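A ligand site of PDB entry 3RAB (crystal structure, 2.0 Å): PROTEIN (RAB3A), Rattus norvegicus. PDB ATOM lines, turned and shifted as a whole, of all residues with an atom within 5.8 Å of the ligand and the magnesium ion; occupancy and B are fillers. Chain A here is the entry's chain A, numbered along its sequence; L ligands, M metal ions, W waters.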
ATOM      1  N   GLY A  12     -12.014 -14.839  -1.035  1.00  0.00           N
ATOM      2  CA  GLY A  12     -10.773 -14.909  -0.293  1.00  0.00           C
ATOM      3  C   GLY A  12     -10.358 -16.365  -0.091  1.00  0.00           C
ATOM      4  O   GLY A  12     -11.146 -17.271  -0.324  1.00  0.00           O
ATOM      5  N   ASN A  13      -9.129 -16.553   0.372  1.00  0.00           N
ATOM      6  CA  ASN A  13      -8.575 -17.891   0.599  1.00  0.00           C
ATOM      7  C   ASN A  13      -9.457 -18.783   1.472  1.00  0.00           C
ATOM      8  O   ASN A  13     -10.243 -18.318   2.305  1.00  0.00           O
ATOM      9  CB  ASN A  13      -7.186 -17.788   1.232  1.00  0.00           C
ATOM     10  CG  ASN A  13      -6.078 -17.661   0.201  1.00  0.00           C
ATOM     11  OD1 ASN A  13      -6.317 -17.298  -0.951  1.00  0.00           O
ATOM     12  ND2 ASN A  13      -4.865 -17.986   0.607  1.00  0.00           N
ATOM     13  N   SER A  14      -9.309 -20.098   1.280  1.00  0.00           N
ATOM     14  CA  SER A  14     -10.049 -21.079   2.050  1.00  0.00           C
ATOM     15  C   SER A  14      -9.655 -20.956   3.521  1.00  0.00           C
ATOM     16  O   SER A  14      -8.487 -20.682   3.827  1.00  0.00           O
ATOM     17  CB  SER A  14      -9.725 -22.487   1.553  1.00  0.00           C
ATOM     18  OG  SER A  14     -10.384 -23.469   2.326  1.00  0.00           O
ATOM     19  N   SER A  15     -10.634 -21.059   4.408  1.00  0.00           N
ATOM     20  CA  SER A  15     -10.458 -21.011   5.868  1.00  0.00           C
ATOM     21  C   SER A  15     -10.290 -19.647   6.519  1.00  0.00           C
ATOM     22  O   SER A  15     -10.021 -19.570   7.728  1.00  0.00           O
ATOM     23  CB  SER A  15      -9.284 -21.897   6.302  1.00  0.00           C
ATOM     24  OG  SER A  15      -8.062 -21.178   6.238  1.00  0.00           O
ATOM     25  N   VAL A  16     -10.453 -18.566   5.768  1.00  0.00           N
ATOM     26  CA  VAL A  16     -10.308 -17.240   6.347  1.00  0.00           C
ATOM     27  C   VAL A  16     -11.511 -16.825   7.193  1.00  0.00           C
ATOM     28  O   VAL A  16     -11.426 -15.917   8.017  1.00  0.00           O
ATOM     29  CB  VAL A  16      -9.980 -16.165   5.281  1.00  0.00           C
ATOM     30  CG1 VAL A  16      -8.618 -16.477   4.652  1.00  0.00           C
ATOM     31  CG2 VAL A  16     -11.053 -16.121   4.218  1.00  0.00           C
ATOM     32  N   GLY A  17     -12.619 -17.540   7.014  1.00  0.00           N
ATOM     33  CA  GLY A  17     -13.836 -17.263   7.765  1.00  0.00           C
ATOM     34  C   GLY A  17     -14.959 -16.592   6.992  1.00  0.00           C
ATOM     35  O   GLY A  17     -15.766 -15.880   7.585  1.00  0.00           O
ATOM     36  N   LYS A  18     -15.040 -16.837   5.681  1.00  0.00           N
ATOM     37  CA  LYS A  18     -16.101 -16.227   4.856  1.00  0.00           C
ATOM     38  C   LYS A  18     -17.480 -16.786   5.197  1.00  0.00           C
ATOM     39  O   LYS A  18     -18.456 -16.045   5.234  1.00  0.00           O
ATOM     40  CB  LYS A  18     -15.814 -16.425   3.365  1.00  0.00           C
ATOM     41  CG  LYS A  18     -14.456 -15.900   2.921  1.00  0.00           C
ATOM     42  CD  LYS A  18     -14.234 -16.104   1.434  1.00  0.00           C
ATOM     43  CE  LYS A  18     -14.212 -17.575   1.029  1.00  0.00           C
ATOM     44  NZ  LYS A  18     -13.116 -18.322   1.696  1.00  0.00           N
ATOM     45  N   THR A  19     -17.576 -18.100   5.370  1.00  0.00           N
ATOM     46  CA  THR A  19     -18.867 -18.693   5.717  1.00  0.00           C
ATOM     47  C   THR A  19     -19.282 -18.267   7.122  1.00  0.00           C
ATOM     48  O   THR A  19     -20.457 -17.975   7.360  1.00  0.00           O
ATOM     49  CB  THR A  19     -18.857 -20.224   5.644  1.00  0.00           C
ATOM     50  OG1 THR A  19     -18.721 -20.610   4.275  1.00  0.00           O
ATOM     51  CG2 THR A  19     -20.183 -20.791   6.161  1.00  0.00           C
ATOM     52  N   SER A  20     -18.334 -18.251   8.041  1.00  0.00           N
ATOM     53  CA  SER A  20     -18.608 -17.858   9.412  1.00  0.00           C
ATOM     54  C   SER A  20     -19.073 -16.405   9.443  1.00  0.00           C
ATOM     55  O   SER A  20     -19.979 -16.046  10.191  1.00  0.00           O
ATOM     56  CB  SER A  20     -17.364 -18.014  10.276  1.00  0.00           C
ATOM     57  OG  SER A  20     -16.931 -19.366  10.265  1.00  0.00           O
ATOM     58  N   PHE A  21     -18.427 -15.576   8.614  1.00  0.00           N
ATOM     59  CA  PHE A  21     -18.768 -14.157   8.534  1.00  0.00           C
ATOM     60  C   PHE A  21     -20.257 -13.999   8.151  1.00  0.00           C
ATOM     61  O   PHE A  21     -20.984 -13.257   8.787  1.00  0.00           O
ATOM     62  CB  PHE A  21     -17.875 -13.460   7.498  1.00  0.00           C
ATOM     63  CG  PHE A  21     -17.657 -11.995   7.774  1.00  0.00           C
ATOM     64  CD1 PHE A  21     -16.803 -11.585   8.796  1.00  0.00           C
ATOM     65  CD2 PHE A  21     -18.269 -11.020   6.990  1.00  0.00           C
ATOM     66  CE1 PHE A  21     -16.556 -10.229   9.020  1.00  0.00           C
ATOM     67  CE2 PHE A  21     -18.036  -9.673   7.207  1.00  0.00           C
ATOM     68  CZ  PHE A  21     -17.172  -9.273   8.225  1.00  0.00           C
ATOM     69  N   PHE A  30     -22.390 -19.087  15.030  1.00  0.00           N
ATOM     70  CA  PHE A  30     -20.988 -19.363  14.773  1.00  0.00           C
ATOM     71  C   PHE A  30     -20.663 -20.797  15.160  1.00  0.00           C
ATOM     72  O   PHE A  30     -21.192 -21.316  16.142  1.00  0.00           O
ATOM     73  CB  PHE A  30     -20.070 -18.399  15.555  1.00  0.00           C
ATOM     74  CG  PHE A  30     -18.598 -18.756  15.494  1.00  0.00           C
ATOM     75  CD1 PHE A  30     -17.826 -18.364  14.405  1.00  0.00           C
ATOM     76  CD2 PHE A  30     -18.005 -19.498  16.501  1.00  0.00           C
ATOM     77  CE1 PHE A  30     -16.474 -18.711  14.332  1.00  0.00           C
ATOM     78  CE2 PHE A  30     -16.663 -19.858  16.439  1.00  0.00           C
ATOM     79  CZ  PHE A  30     -15.899 -19.462  15.346  1.00  0.00           C
ATOM     80  N   THR A  31     -19.848 -21.438  14.342  1.00  0.00           N
ATOM     81  CA  THR A  31     -19.417 -22.806  14.576  1.00  0.00           C
ATOM     82  C   THR A  31     -17.901 -22.903  14.473  1.00  0.00           C
ATOM     83  O   THR A  31     -17.307 -22.350  13.544  1.00  0.00           O
ATOM     84  CB  THR A  31     -20.040 -23.794  13.566  1.00  0.00           C
ATOM     85  OG1 THR A  31     -19.561 -25.114  13.852  1.00  0.00           O
ATOM     86  CG2 THR A  31     -19.652 -23.435  12.143  1.00  0.00           C
ATOM     87  N   PRO A  32     -17.255 -23.498  15.491  1.00  0.00           N
ATOM     88  CA  PRO A  32     -15.801 -23.671  15.513  1.00  0.00           C
ATOM     89  C   PRO A  32     -15.365 -24.681  14.453  1.00  0.00           C
ATOM     90  O   PRO A  32     -14.228 -24.656  14.008  1.00  0.00           O
ATOM     91  CB  PRO A  32     -15.557 -24.219  16.931  1.00  0.00           C
ATOM     92  CG  PRO A  32     -16.675 -23.648  17.718  1.00  0.00           C
ATOM     93  CD  PRO A  32     -17.840 -23.850  16.800  1.00  0.00           C
ATOM     94  N   ALA A  33     -16.315 -25.482  13.963  1.00  0.00           N
ATOM     95  CA  ALA A  33     -16.028 -26.507  12.962  1.00  0.00           C
ATOM     96  C   ALA A  33     -15.681 -25.892  11.614  1.00  0.00           C
ATOM     97  O   ALA A  33     -16.191 -24.837  11.244  1.00  0.00           O
ATOM     98  CB  ALA A  33     -17.209 -27.430  12.808  1.00  0.00           C
ATOM     99  N   PHE A  34     -14.825 -26.586  10.865  1.00  0.00           N
ATOM    100  CA  PHE A  34     -14.422 -26.130   9.544  1.00  0.00           C
ATOM    101  C   PHE A  34     -15.082 -27.020   8.506  1.00  0.00           C
ATOM    102  O   PHE A  34     -14.682 -28.171   8.318  1.00  0.00           O
ATOM    103  CB  PHE A  34     -12.899 -26.174   9.400  1.00  0.00           C
ATOM    104  CG  PHE A  34     -12.387 -25.637   8.081  1.00  0.00           C
ATOM    105  CD1 PHE A  34     -13.256 -25.022   7.168  1.00  0.00           C
ATOM    106  CD2 PHE A  34     -11.042 -25.746   7.751  1.00  0.00           C
ATOM    107  CE1 PHE A  34     -12.792 -24.542   5.958  1.00  0.00           C
ATOM    108  CE2 PHE A  34     -10.573 -25.265   6.528  1.00  0.00           C
ATOM    109  CZ  PHE A  34     -11.452 -24.657   5.633  1.00  0.00           C
ATOM    110  N   VAL A  35     -16.178 -26.546   7.930  1.00  0.00           N
ATOM    111  CA  VAL A  35     -16.885 -27.291   6.914  1.00  0.00           C
ATOM    112  C   VAL A  35     -16.721 -26.487   5.625  1.00  0.00           C
ATOM    113  O   VAL A  35     -17.465 -25.539   5.360  1.00  0.00           O
ATOM    114  CB  VAL A  35     -18.390 -27.432   7.261  1.00  0.00           C
ATOM    115  CG1 VAL A  35     -19.027 -28.458   6.358  1.00  0.00           C
ATOM    116  CG2 VAL A  35     -18.562 -27.840   8.705  1.00  0.00           C
ATOM    117  N   SER A  36     -15.687 -26.844   4.855  1.00  0.00           N
ATOM    118  CA  SER A  36     -15.359 -26.181   3.608  1.00  0.00           C
ATOM    119  C   SER A  36     -16.528 -26.081   2.613  1.00  0.00           C
ATOM    120  O   SER A  36     -17.291 -27.038   2.436  1.00  0.00           O
ATOM    121  CB  SER A  36     -14.147 -26.878   2.964  1.00  0.00           C
ATOM    122  OG  SER A  36     -13.598 -26.112   1.899  1.00  0.00           O
ATOM    123  N   THR A  37     -16.685 -24.902   2.013  1.00  0.00           N
ATOM    124  CA  THR A  37     -17.749 -24.656   1.044  1.00  0.00           C
ATOM    125  C   THR A  37     -17.436 -25.306  -0.311  1.00  0.00           C
ATOM    126  O   THR A  37     -16.336 -25.181  -0.838  1.00  0.00           O
ATOM    127  CB  THR A  37     -17.995 -23.135   0.848  1.00  0.00           C
ATOM    128  OG1 THR A  37     -18.349 -22.558   2.106  1.00  0.00           O
ATOM    129  CG2 THR A  37     -19.129 -22.874  -0.135  1.00  0.00           C
ATOM    130  N   VAL A  38     -18.411 -26.037  -0.833  1.00  0.00           N
ATOM    131  CA  VAL A  38     -18.308 -26.714  -2.109  1.00  0.00           C
ATOM    132  C   VAL A  38     -18.770 -25.792  -3.231  1.00  0.00           C
ATOM    133  O   VAL A  38     -19.965 -25.625  -3.458  1.00  0.00           O
ATOM    134  CB  VAL A  38     -19.174 -28.002  -2.125  1.00  0.00           C
ATOM    135  CG1 VAL A  38     -19.016 -28.736  -3.456  1.00  0.00           C
ATOM    136  CG2 VAL A  38     -18.809 -28.911  -0.952  1.00  0.00           C
ATOM    137  N   ASP A  60     -21.667 -16.774  -0.899  1.00  0.00           N
ATOM    138  CA  ASP A  60     -20.516 -17.214  -0.130  1.00  0.00           C
ATOM    139  C   ASP A  60     -19.695 -18.147  -1.009  1.00  0.00           C
ATOM    140  O   ASP A  60     -20.061 -19.303  -1.230  1.00  0.00           O
ATOM    141  CB  ASP A  60     -21.054 -17.927   1.111  1.00  0.00           C
ATOM    142  CG  ASP A  60     -19.964 -18.529   1.956  1.00  0.00           C
ATOM    143  OD1 ASP A  60     -18.815 -18.042   1.922  1.00  0.00           O
ATOM    144  OD2 ASP A  60     -20.285 -19.505   2.659  1.00  0.00           O
ATOM    145  N   THR A  61     -18.595 -17.634  -1.554  1.00  0.00           N
ATOM    146  CA  THR A  61     -17.737 -18.423  -2.444  1.00  0.00           C
ATOM    147  C   THR A  61     -16.735 -19.316  -1.713  1.00  0.00           C
ATOM    148  O   THR A  61     -16.326 -19.021  -0.600  1.00  0.00           O
ATOM    149  CB  THR A  61     -16.933 -17.522  -3.404  1.00  0.00           C
ATOM    150  OG1 THR A  61     -15.944 -16.800  -2.668  1.00  0.00           O
ATOM    151  CG2 THR A  61     -17.850 -16.547  -4.134  1.00  0.00           C
ATOM    152  N   ALA A  62     -16.357 -20.403  -2.377  1.00  0.00           N
ATOM    153  CA  ALA A  62     -15.354 -21.319  -1.847  1.00  0.00           C
ATOM    154  C   ALA A  62     -13.996 -20.658  -2.079  1.00  0.00           C
ATOM    155  O   ALA A  62     -13.801 -19.980  -3.098  1.00  0.00           O
ATOM    156  CB  ALA A  62     -15.433 -22.640  -2.582  1.00  0.00           C
ATOM    157  N   GLY A  63     -13.078 -20.836  -1.132  1.00  0.00           N
ATOM    158  CA  GLY A  63     -11.751 -20.246  -1.256  1.00  0.00           C
ATOM    159  C   GLY A  63     -10.764 -21.081  -2.053  1.00  0.00           C
ATOM    160  O   GLY A  63      -9.840 -20.525  -2.665  1.00  0.00           O
ATOM    161  N   GLN A  64     -10.932 -22.396  -2.050  1.00  0.00           N
ATOM    162  CA  GLN A  64     -10.042 -23.310  -2.759  1.00  0.00           C
ATOM    163  C   GLN A  64      -9.958 -23.042  -4.261  1.00  0.00           C
ATOM    164  O   GLN A  64     -10.966 -22.821  -4.937  1.00  0.00           O
ATOM    165  CB  GLN A  64     -10.446 -24.765  -2.484  1.00  0.00           C
ATOM    166  CG  GLN A  64     -10.273 -25.148  -1.022  1.00  0.00           C
ATOM    167  CD  GLN A  64     -10.638 -26.599  -0.722  1.00  0.00           C
ATOM    168  OE1 GLN A  64      -9.821 -27.359  -0.221  1.00  0.00           O
ATOM    169  NE2 GLN A  64     -11.875 -26.963  -1.022  1.00  0.00           N
ATOM    170  N   ASN A 118     -10.309 -10.747   8.851  1.00  0.00           N
ATOM    171  CA  ASN A 118     -11.140 -11.464   9.828  1.00  0.00           C
ATOM    172  C   ASN A 118     -10.318 -12.160  10.934  1.00  0.00           C
ATOM    173  O   ASN A 118      -9.081 -12.266  10.842  1.00  0.00           O
ATOM    174  CB  ASN A 118     -12.043 -12.463   9.113  1.00  0.00           C
ATOM    175  CG  ASN A 118     -13.034 -13.139  10.039  1.00  0.00           C
ATOM    176  OD1 ASN A 118     -13.641 -12.500  10.892  1.00  0.00           O
ATOM    177  ND2 ASN A 118     -13.202 -14.452   9.874  1.00  0.00           N
ATOM    178  N   LYS A 119     -11.020 -12.658  11.957  1.00  0.00           N
ATOM    179  CA  LYS A 119     -10.426 -13.345  13.112  1.00  0.00           C
ATOM    180  C   LYS A 119      -9.565 -12.405  13.976  1.00  0.00           C
ATOM    181  O   LYS A 119      -8.562 -12.845  14.559  1.00  0.00           O
ATOM    182  CB  LYS A 119      -9.587 -14.555  12.679  1.00  0.00           C
ATOM    183  CG  LYS A 119     -10.321 -15.536  11.775  1.00  0.00           C
ATOM    184  CD  LYS A 119      -9.530 -16.818  11.604  1.00  0.00           C
ATOM    185  CE  LYS A 119     -10.195 -17.737  10.601  1.00  0.00           C
ATOM    186  NZ  LYS A 119      -9.378 -18.958  10.381  1.00  0.00           N
ATOM    187  N   CYS A 120      -9.975 -11.143  14.086  1.00  0.00           N
ATOM    188  CA  CYS A 120      -9.210 -10.174  14.872  1.00  0.00           C
ATOM    189  C   CYS A 120      -9.259 -10.477  16.364  1.00  0.00           C
ATOM    190  O   CYS A 120      -8.584  -9.816  17.164  1.00  0.00           O
ATOM    191  CB  CYS A 120      -9.669  -8.732  14.590  1.00  0.00           C
ATOM    192  SG  CYS A 120     -11.319  -8.304  15.192  1.00  0.00           S
ATOM    193  N   ASP A 121     -10.071 -11.461  16.734  1.00  0.00           N
ATOM    194  CA  ASP A 121     -10.187 -11.889  18.133  1.00  0.00           C
ATOM    195  C   ASP A 121      -8.934 -12.662  18.504  1.00  0.00           C
ATOM    196  O   ASP A 121      -8.580 -12.782  19.682  1.00  0.00           O
ATOM    197  CB  ASP A 121     -11.428 -12.771  18.315  1.00  0.00           C
ATOM    198  CG  ASP A 121     -11.449 -13.939  17.356  1.00  0.00           C
ATOM    199  OD1 ASP A 121     -11.925 -13.765  16.220  1.00  0.00           O
ATOM    200  OD2 ASP A 121     -10.983 -15.026  17.737  1.00  0.00           O
ATOM    201  N   MET A 122      -8.265 -13.208  17.489  1.00  0.00           N
ATOM    202  CA  MET A 122      -7.031 -13.986  17.645  1.00  0.00           C
ATOM    203  C   MET A 122      -5.831 -13.050  17.738  1.00  0.00           C
ATOM    204  O   MET A 122      -4.859 -13.188  16.995  1.00  0.00           O
ATOM    205  CB  MET A 122      -6.841 -14.884  16.422  1.00  0.00           C
ATOM    206  CG  MET A 122      -7.967 -15.846  16.121  1.00  0.00           C
ATOM    207  SD  MET A 122      -7.706 -17.423  16.930  1.00  0.00           S
ATOM    208  CE  MET A 122      -8.747 -17.224  18.253  1.00  0.00           C
ATOM    209  N   ALA A 147     -12.188  -7.658  11.512  1.00  0.00           N
ATOM    210  CA  ALA A 147     -13.398  -8.128  12.174  1.00  0.00           C
ATOM    211  C   ALA A 147     -13.253  -9.504  12.778  1.00  0.00           C
ATOM    212  O   ALA A 147     -12.217 -10.141  12.685  1.00  0.00           O
ATOM    213  CB  ALA A 147     -14.573  -8.106  11.190  1.00  0.00           C
ATOM    214  N   SER A 148     -14.343  -9.952  13.400  1.00  0.00           N
ATOM    215  CA  SER A 148     -14.394 -11.266  14.038  1.00  0.00           C
ATOM    216  C   SER A 148     -15.794 -11.866  13.923  1.00  0.00           C
ATOM    217  O   SER A 148     -16.752 -11.373  14.522  1.00  0.00           O
ATOM    218  CB  SER A 148     -13.997 -11.154  15.517  1.00  0.00           C
ATOM    219  OG  SER A 148     -14.067 -12.420  16.141  1.00  0.00           O
ATOM    220  N   ALA A 149     -15.907 -12.893  13.090  1.00  0.00           N
ATOM    221  CA  ALA A 149     -17.169 -13.598  12.923  1.00  0.00           C
ATOM    222  C   ALA A 149     -17.482 -14.283  14.253  1.00  0.00           C
ATOM    223  O   ALA A 149     -18.625 -14.376  14.663  1.00  0.00           O
ATOM    224  CB  ALA A 149     -17.049 -14.622  11.813  1.00  0.00           C
ATOM    225  N   LYS A 150     -16.429 -14.737  14.926  1.00  0.00           N
ATOM    226  CA  LYS A 150     -16.568 -15.412  16.215  1.00  0.00           C
ATOM    227  C   LYS A 150     -17.102 -14.503  17.314  1.00  0.00           C
ATOM    228  O   LYS A 150     -18.109 -14.815  17.945  1.00  0.00           O
ATOM    229  CB  LYS A 150     -15.225 -16.003  16.661  1.00  0.00           C
ATOM    230  CG  LYS A 150     -15.276 -16.674  18.026  1.00  0.00           C
ATOM    231  CD  LYS A 150     -13.892 -17.048  18.504  1.00  0.00           C
ATOM    232  CE  LYS A 150     -13.909 -17.465  19.961  1.00  0.00           C
ATOM    233  NZ  LYS A 150     -14.312 -16.379  20.883  1.00  0.00           N
ATOM    234  N   ASP A 151     -16.416 -13.381  17.549  1.00  0.00           N
ATOM    235  CA  ASP A 151     -16.829 -12.450  18.608  1.00  0.00           C
ATOM    236  C   ASP A 151     -17.840 -11.408  18.155  1.00  0.00           C
ATOM    237  O   ASP A 151     -18.143 -10.465  18.901  1.00  0.00           O
ATOM    238  CB  ASP A 151     -15.603 -11.756  19.221  1.00  0.00           C
ATOM    239  CG  ASP A 151     -14.797 -12.678  20.136  1.00  0.00           C
ATOM    240  OD1 ASP A 151     -15.202 -13.835  20.351  1.00  0.00           O
ATOM    241  OD2 ASP A 151     -13.761 -12.218  20.660  1.00  0.00           O
HETATM  242  P1  LIG L   1     -13.763 -22.168   2.510  1.00  0.00           P
HETATM  243  O1  LIG L   1     -12.828 -23.308   2.551  1.00  0.00           O
HETATM  244  O2  LIG L   1     -15.174 -22.564   2.397  1.00  0.00           O
HETATM  245  O3  LIG L   1     -13.361 -21.068   1.608  1.00  0.00           O
HETATM  246  N1  LIG L   1     -13.623 -21.533   4.035  1.00  0.00           N
HETATM  247  P2  LIG L   1     -14.141 -20.156   4.794  1.00  0.00           P
HETATM  248  O4  LIG L   1     -13.248 -19.051   4.393  1.00  0.00           O
HETATM  249  O5  LIG L   1     -15.579 -20.018   4.609  1.00  0.00           O
HETATM  250  O6  LIG L   1     -13.923 -20.387   6.379  1.00  0.00           O
HETATM  251  P3  LIG L   1     -14.966 -20.903   7.496  1.00  0.00           P
HETATM  252  O7  LIG L   1     -16.007 -19.880   7.752  1.00  0.00           O
HETATM  253  O8  LIG L   1     -15.356 -22.294   7.180  1.00  0.00           O
HETATM  254  O9  LIG L   1     -13.944 -20.914   8.722  1.00  0.00           O
HETATM  255  C1  LIG L   1     -12.776 -21.716   8.780  1.00  0.00           C
HETATM  256  C2  LIG L   1     -12.411 -21.895  10.238  1.00  0.00           C
HETATM  257  O10 LIG L   1     -12.141 -20.630  10.845  1.00  0.00           O
HETATM  258  C3  LIG L   1     -13.561 -22.481  11.021  1.00  0.00           C
HETATM  259  O11 LIG L   1     -12.992 -23.443  11.896  1.00  0.00           O
HETATM  260  C4  LIG L   1     -14.188 -21.292  11.775  1.00  0.00           C
HETATM  261  O12 LIG L   1     -14.643 -21.648  13.077  1.00  0.00           O
HETATM  262  C5  LIG L   1     -13.013 -20.363  11.950  1.00  0.00           C
HETATM  263  N2  LIG L   1     -13.361 -18.927  12.076  1.00  0.00           N
HETATM  264  C6  LIG L   1     -14.089 -18.146  11.213  1.00  0.00           C
HETATM  265  N3  LIG L   1     -14.182 -16.893  11.573  1.00  0.00           N
HETATM  266  C7  LIG L   1     -13.464 -16.826  12.765  1.00  0.00           C
HETATM  267  C8  LIG L   1     -13.218 -15.717  13.627  1.00  0.00           C
HETATM  268  O13 LIG L   1     -13.585 -14.553  13.521  1.00  0.00           O
HETATM  269  N4  LIG L   1     -12.440 -16.086  14.723  1.00  0.00           N
HETATM  270  C9  LIG L   1     -11.960 -17.354  14.981  1.00  0.00           C
HETATM  271  N5  LIG L   1     -11.233 -17.497  16.086  1.00  0.00           N
HETATM  272  N6  LIG L   1     -12.206 -18.401  14.160  1.00  0.00           N
HETATM  273  C10 LIG L   1     -12.960 -18.068  13.080  1.00  0.00           C
HETATM  274 MG    MG M   1     -16.836 -21.365   3.302  1.00  0.00          MG
HETATM  275  O   HOH W   1     -16.737 -23.048   5.015  1.00  0.00           O
HETATM  276  O   HOH W   2     -16.701 -19.632   1.736  1.00  0.00           O
HETATM  277  O   HOH W   3      -9.644 -19.875  13.161  1.00  0.00           O
HETATM  278  O   HOH W   4     -13.296 -23.993  -0.437  1.00  0.00           O
HETATM  279  O   HOH W   5     -16.928 -23.698   8.805  1.00  0.00           O
HETATM  280  O   HOH W   6     -13.126 -20.359  16.062  1.00  0.00           O
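The backbone NH (N) of Thr 19 sits at hydrogen-bond distance from an oxygen (O7) of the ligand (3.4 Å). N of Thr 37 sits close to O2 of the ligand. O1 of the ligand lies within hydrogen-bond range of OG of Ser 14 (2.5 Å). The backbone NH (N) of Ser 20 sits at hydrogen-bond distance from an oxygen (O7) of the ligand, at 2.9 Å. The side-chain hydroxyl (OG) of Ser 20 sits at hydrogen-bond distance from an oxygen (O7) of the ligand, at 2.7 Å. An oxygen (O11) of the ligand is in hydrogen-bond range of the backbone carbonyl oxygen (O) of Pro 32, at 2.7 Å. An oxygen (O4) of the ligand lies within hydrogen-bond range of the backbone NH of Lys 18 (3.1 Å). NZ of Lys 18 is in salt-bridge range of O3 of the ligand (2.8 Å). The backbone NH of Gly 63 is in hydrogen-bond range of an oxygen (O3) of the ligand (2.8 Å). O of Thr 31 lies within hydrogen-bond range of O12 of the ligand (2.8 Å). The side-chain carboxylate (OD1) of Asp 121 sits at hydrogen-bond distance from a nitrogen (N4) of the ligand (2.8 Å). N of Ala 149 is in hydrogen-bond range of O13 of the ligand (2.9 Å). O1 of the ligand sits at hydrogen-bond distance from OG of Ser 36, 3.0 Å away. O4 of the ligand lies within hydrogen-bond range of N of Ser 15. N of Gly 17 sits at hydrogen-bond distance from O4 of the ligand (3.1 Å). A nitrogen (N3) of the ligand is in hydrogen-bond range of the side-chain amide nitrogen (ND2) of Asn 118 (3.1 Å). An oxygen (O4) of the ligand sits at hydrogen-bond distance from the backbone NH of Val 16 (3.2 Å). An oxygen (O13) of the ligand is in hydrogen-bond range of the backbone NH (N) of Lys 150, 3.2 Å away. O10 of the ligand sits at hydrogen-bond distance from NZ of Lys 119. The side-chain sulfur of Met 122 sits close to a nitrogen (N5) of the ligand, 3.6 Å away. The side-chain hydroxyl (OG) of Ser 148 sits at hydrogen-bond distance from an oxygen (O13) of the ligand.
OG1 of Thr 19 lies close to OD2 of Asp 60 (2.5 Å). O of Asn 13 sits at hydrogen-bond distance from NZ of Lys 18 (2.9 Å). The side-chain hydroxyl of Ser 148 lies within hydrogen-bond range of the side-chain carboxylate of Asp 121 (2.5 Å). OD1 of Asn 118 lies within hydrogen-bond range of N of Ala 149. The side-chain amide nitrogen (NE2) of Gln 64 sits at hydrogen-bond distance from the side-chain hydroxyl (OG) of Ser 36 (3.5 Å). ND2 of Asn 118 sits at hydrogen-bond distance from O of Val 16 (3.0 Å). The backbone carbonyl oxygen (O) of Ala 147 lies close to the side-chain amide oxygen (OD1) of Asn 118, 3.3 Å away. OD1 of Asp 151 is in salt-bridge range of NZ of Lys 150, 2.7 Å away.
Residues that only touch the ligand: Phe 30, Phe 34, Ala 33, Asn 13 and Ala 62. Of the 34 residues printed, 24 come within 4 Å of the ligand.
Merely in contact with the magnesium ion: Asp 60 (3.97 Å). Of the 34 residues printed, 3 come within 4 Å of the magnesium ion. The nearest printed residue that does not touch the magnesium ion is Thr 61 (4.6 Å).
O2 of the ligand is bound to the magnesium ion. OG1 of Thr 19 binds the magnesium ion, at 2.3 Å. The magnesium ion is bound by O5 of the ligand (2.3 Å). OG1 of Thr 37 binds the magnesium ion (2.3 Å). The magnesium ion is bound by water W2 (2.3 Å). Water W1 is bound to the magnesium ion (2.4 Å).
Water W2 lies within hydrogen-bond range of O of Thr 61 (2.4 Å) and OD1 of Asp 60 (2.7 Å). Water W1 lies within hydrogen-bond range of O of Val 35 and O8 of the ligand. Water W5 lies within hydrogen-bond range of O8 of the ligand (2.7 Å), O of Ala 33 (2.8 Å) and N of Val 35 (3.1 Å). Water W4 lies within hydrogen-bond range of O1 of the ligand, OG of Ser 36, N of Gly 63, N of Gln 64 and O of Thr 37. Water W3 bridges NZ of Lys 119 (2.9 Å) and N6 of the ligand (3.1 Å).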
